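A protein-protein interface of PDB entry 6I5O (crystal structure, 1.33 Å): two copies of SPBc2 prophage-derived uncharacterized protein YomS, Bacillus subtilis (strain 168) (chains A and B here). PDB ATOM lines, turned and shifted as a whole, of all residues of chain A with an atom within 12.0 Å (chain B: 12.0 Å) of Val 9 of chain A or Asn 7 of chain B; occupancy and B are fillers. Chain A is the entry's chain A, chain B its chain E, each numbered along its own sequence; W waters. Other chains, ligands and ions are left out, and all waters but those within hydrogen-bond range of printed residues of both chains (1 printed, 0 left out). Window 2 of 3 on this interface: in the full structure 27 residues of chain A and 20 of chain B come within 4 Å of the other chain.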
ATOM      1  N   ASN A   7      -4.426  16.240 -25.519  1.00  0.00           N
ATOM      2  CA  ASN A   7      -3.558  15.188 -26.119  1.00  0.00           C
ATOM      3  C   ASN A   7      -3.243  14.040 -25.148  1.00  0.00           C
ATOM      4  O   ASN A   7      -2.532  14.257 -24.191  1.00  0.00           O
ATOM      5  CB  ASN A   7      -2.225  15.803 -26.506  1.00  0.00           C
ATOM      6  CG  ASN A   7      -1.759  15.234 -27.818  1.00  0.00           C
ATOM      7  OD1 ASN A   7      -2.260  15.649 -28.871  1.00  0.00           O
ATOM      8  ND2 ASN A   7      -0.881  14.246 -27.758  1.00  0.00           N
ATOM      9  N   VAL A   8      -3.714  12.845 -25.408  1.00  0.00           N
ATOM     10  CA  VAL A   8      -3.551  11.687 -24.505  1.00  0.00           C
ATOM     11  C   VAL A   8      -2.417  10.836 -25.031  1.00  0.00           C
ATOM     12  O   VAL A   8      -2.450  10.522 -26.239  1.00  0.00           O
ATOM     13  CB  VAL A   8      -4.848  10.873 -24.363  1.00  0.00           C
ATOM     14  CG1 VAL A   8      -4.650   9.651 -23.482  1.00  0.00           C
ATOM     15  CG2 VAL A   8      -5.985  11.710 -23.846  1.00  0.00           C
ATOM     16  N   VAL A   9      -1.513  10.429 -24.193  1.00  0.00           N
ATOM     17  CA  VAL A   9      -0.405   9.531 -24.547  1.00  0.00           C
ATOM     18  C   VAL A   9      -0.393   8.348 -23.612  1.00  0.00           C
ATOM     19  O   VAL A   9      -0.637   8.514 -22.380  1.00  0.00           O
ATOM     20  CB  VAL A   9       0.969  10.242 -24.565  1.00  0.00           C
ATOM     21  CG1 VAL A   9       0.969  11.338 -25.618  1.00  0.00           C
ATOM     22  CG2 VAL A   9       1.366  10.753 -23.225  1.00  0.00           C
ATOM     23  N   ILE A  10      -0.052   7.199 -24.152  1.00  0.00           N
ATOM     24  CA  ILE A  10       0.212   5.984 -23.363  1.00  0.00           C
ATOM     25  C   ILE A  10       1.670   6.018 -23.012  1.00  0.00           C
ATOM     26  O   ILE A  10       2.531   6.102 -23.921  1.00  0.00           O
ATOM     27  CB  ILE A  10      -0.134   4.725 -24.202  1.00  0.00           C
ATOM     28  CG1 ILE A  10      -1.646   4.702 -24.425  1.00  0.00           C
ATOM     29  CG2 ILE A  10       0.416   3.476 -23.542  1.00  0.00           C
ATOM     30  CD1 ILE A  10      -2.056   3.848 -25.621  1.00  0.00           C
ATOM     31  N   THR A  11       2.008   5.919 -21.742  1.00  0.00           N
ATOM     32  CA  THR A  11       3.387   6.041 -21.282  1.00  0.00           C
ATOM     33  C   THR A  11       3.995   4.718 -20.936  1.00  0.00           C
ATOM     34  O   THR A  11       3.355   3.910 -20.205  1.00  0.00           O
ATOM     35  CB  THR A  11       3.511   6.986 -20.080  1.00  0.00           C
ATOM     36  OG1 THR A  11       2.699   6.532 -19.006  1.00  0.00           O
ATOM     37  CG2 THR A  11       3.083   8.378 -20.462  1.00  0.00           C
ATOM     38  N   ILE A  12       5.215   4.461 -21.405  1.00  0.00           N
ATOM     39  CA  ILE A  12       5.984   3.274 -20.998  1.00  0.00           C
ATOM     40  C   ILE A  12       7.396   3.740 -20.646  1.00  0.00           C
ATOM     41  O   ILE A  12       7.861   4.773 -21.134  1.00  0.00           O
ATOM     42  CB  ILE A  12       6.027   2.249 -22.148  1.00  0.00           C
ATOM     43  CG1 ILE A  12       6.766   2.781 -23.379  1.00  0.00           C
ATOM     44  CG2 ILE A  12       4.610   1.798 -22.495  1.00  0.00           C
ATOM     45  CD1 ILE A  12       7.041   1.716 -24.447  1.00  0.00           C
ATOM     46  N   PRO A  13       8.062   2.997 -19.762  1.00  0.00           N
ATOM     47  CA  PRO A  13       9.434   3.357 -19.395  1.00  0.00           C
ATOM     48  C   PRO A  13      10.402   2.969 -20.489  1.00  0.00           C
ATOM     49  O   PRO A  13      10.158   2.062 -21.286  1.00  0.00           O
ATOM     50  CB  PRO A  13       9.711   2.492 -18.172  1.00  0.00           C
ATOM     51  CG  PRO A  13       8.819   1.294 -18.370  1.00  0.00           C
ATOM     52  CD  PRO A  13       7.594   1.811 -19.028  1.00  0.00           C
ATOM     53  N   ASN B   7      -1.373   6.489 -29.111  1.00  0.00           N
ATOM     54  CA  ASN B   7      -0.024   7.153 -29.236  1.00  0.00           C
ATOM     55  C   ASN B   7       0.905   6.874 -28.046  1.00  0.00           C
ATOM     56  O   ASN B   7       0.657   7.359 -26.947  1.00  0.00           O
ATOM     57  CB  ASN B   7      -0.160   8.665 -29.267  1.00  0.00           C
ATOM     58  CG  ASN B   7       0.778   9.219 -30.300  1.00  0.00           C
ATOM     59  OD1 ASN B   7       0.484   9.137 -31.508  1.00  0.00           O
ATOM     60  ND2 ASN B   7       1.906   9.710 -29.829  1.00  0.00           N
ATOM     61  N   VAL B   8       1.926   6.084 -28.238  1.00  0.00           N
ATOM     62  CA  VAL B   8       2.752   5.527 -27.139  1.00  0.00           C
ATOM     63  C   VAL B   8       4.020   6.341 -27.067  1.00  0.00           C
ATOM     64  O   VAL B   8       4.652   6.568 -28.151  1.00  0.00           O
ATOM     65  CB  VAL B   8       3.043   4.043 -27.366  1.00  0.00           C
ATOM     66  CG1 VAL B   8       3.977   3.500 -26.306  1.00  0.00           C
ATOM     67  CG2 VAL B   8       1.784   3.228 -27.474  1.00  0.00           C
ATOM     68  N   VAL B   9       4.444   6.742 -25.904  1.00  0.00           N
ATOM     69  CA  VAL B   9       5.717   7.479 -25.713  1.00  0.00           C
ATOM     70  C   VAL B   9       6.490   6.768 -24.625  1.00  0.00           C
ATOM     71  O   VAL B   9       5.925   6.266 -23.632  1.00  0.00           O
ATOM     72  CB  VAL B   9       5.518   8.963 -25.369  1.00  0.00           C
ATOM     73  CG1 VAL B   9       4.785   9.651 -26.513  1.00  0.00           C
ATOM     74  CG2 VAL B   9       4.807   9.168 -24.022  1.00  0.00           C
ATOM     75  N   ILE B  10       7.791   6.736 -24.813  1.00  0.00           N
ATOM     76  CA  ILE B  10       8.734   6.300 -23.769  1.00  0.00           C
ATOM     77  C   ILE B  10       9.054   7.504 -22.921  1.00  0.00           C
ATOM     78  O   ILE B  10       9.494   8.537 -23.451  1.00  0.00           O
ATOM     79  CB  ILE B  10       9.997   5.732 -24.447  1.00  0.00           C
ATOM     80  CG1 ILE B  10       9.625   4.494 -25.257  1.00  0.00           C
ATOM     81  CG2 ILE B  10      11.096   5.484 -23.434  1.00  0.00           C
ATOM     82  CD1 ILE B  10      10.715   4.042 -26.221  1.00  0.00           C
ATOM     83  N   THR B  11       8.890   7.392 -21.621  1.00  0.00           N
ATOM     84  CA  THR B  11       9.080   8.531 -20.692  1.00  0.00           C
ATOM     85  C   THR B  11      10.419   8.435 -19.987  1.00  0.00           C
ATOM     86  O   THR B  11      10.745   7.379 -19.431  1.00  0.00           O
ATOM     87  CB  THR B  11       7.910   8.670 -19.716  1.00  0.00           C
ATOM     88  OG1 THR B  11       7.800   7.479 -18.933  1.00  0.00           O
ATOM     89  CG2 THR B  11       6.627   8.958 -20.456  1.00  0.00           C
ATOM     90  N   ILE B  12      11.128   9.552 -19.890  1.00  0.00           N
ATOM     91  CA  ILE B  12      12.333   9.672 -19.047  1.00  0.00           C
ATOM     92  C   ILE B  12      12.202  10.963 -18.257  1.00  0.00           C
ATOM     93  O   ILE B  12      11.555  11.914 -18.727  1.00  0.00           O
ATOM     94  CB  ILE B  12      13.628   9.634 -19.894  1.00  0.00           C
ATOM     95  CG1 ILE B  12      13.722  10.848 -20.819  1.00  0.00           C
ATOM     96  CG2 ILE B  12      13.753   8.342 -20.657  1.00  0.00           C
ATOM     97  CD1 ILE B  12      15.089  10.963 -21.531  1.00  0.00           C
HETATM   98  O   HOH W   1       6.543   5.171 -18.060  1.00  0.00           O
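O of Asn 7 of chain B is in hydrogen-bond range of N of Ile 10 of chain A, at 2.9 Å. O of Ile 10 of chain A lies within hydrogen-bond range of N of Val 9 of chain B, at 2.8 Å. The backbone carbonyl oxygen (O) of Val 9 of chain B is in hydrogen-bond range of the backbone NH (N) of Ile 12 of chain A (3.0 Å). The backbone carbonyl oxygen (O) of Ile 12 of chain A lies within hydrogen-bond range of the backbone NH (N) of Thr 11 of chain B, 2.9 Å away.
Among the printed residues, merely in contact across the chains: Ile 12 of chain A with Ile 10 of chain B, Ile 10 of chain A with Val 8 of chain B, Val 9 of chain A with Asn 7 of chain B, Thr 11 of chain A with Val 9 of chain B, Thr 11 of chain A with Thr 11 of chain B, Val 9 of chain A with Val 9 of chain B and Pro 13 of chain A with Ile 10 of chain B.
Of chain B, only Asn 7 and Val 9 come within 4 Å of Val 9 of chain A. Of the printed residues of chain A, Asn 7 of chain B touches Val 9 and Ile 10. No residue of chain B comes within 4 Å of Asn 7 of chain A. Thr 11 of chain A touches two residues of chain B. Val 9 of chain B touches four residues of chain A. Of the printed residues of chain A, Val 8 of chain B touches Ile 10 (3.3 Å). Of the printed residues of chain A, Thr 11 of chain B touches Thr 11 and Ile 12. Ile 12 of chain B touches none of the printed residues of chain A.
Of the 6 printed residues of chain B, 5 touch a printed residue of chain A. Hydrophobic or aromatic side chains of chain B within 4 Å of the printed part of chain A: Val 8, Val 9 and Ile 10. Of the 7 printed residues of chain A, 5 touch a printed residue of chain B. Printed residues of chain A that touch a printed residue of chain B: Val 9, Ile 10, Thr 11, Ile 12 and Pro 13. Hydrophobic or aromatic side chains of chain A within 4 Å of the printed part of chain B: Val 9, Ile 10 and Ile 12. Among the printed residues, no Asp or Glu carboxylate lies within 4 Å of a Lys or Arg side-chain nitrogen of the other chain.
Val 9 of chain A touches its own counterpart, Val 9 of chain B. Thr 11 of chain A touches Val 9 of chain B, but with the chains exchanged Val 9 of chain A does not touch Thr 11 of chain B (6.2 Å). Thr 11 of chain B touches its own counterpart, Thr 11 of chain A. Ile 12 of chain A touches Val 9 of chain B, but with the chains exchanged Val 9 of chain A does not touch Ile 12 of chain B (10.4 Å). Positions printed for both chains: 7, 8, 9, 10, 11 and 12. Of the 11 pairs that touch across the chains among the printed residues, 2 have their exchanged pair printed and touching as well.
Water W1 bridges the side-chain hydroxyl of Thr 11 of chain B (2.8 Å) and the backbone carbonyl oxygen of Ile 12 of chain A (3.4 Å).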
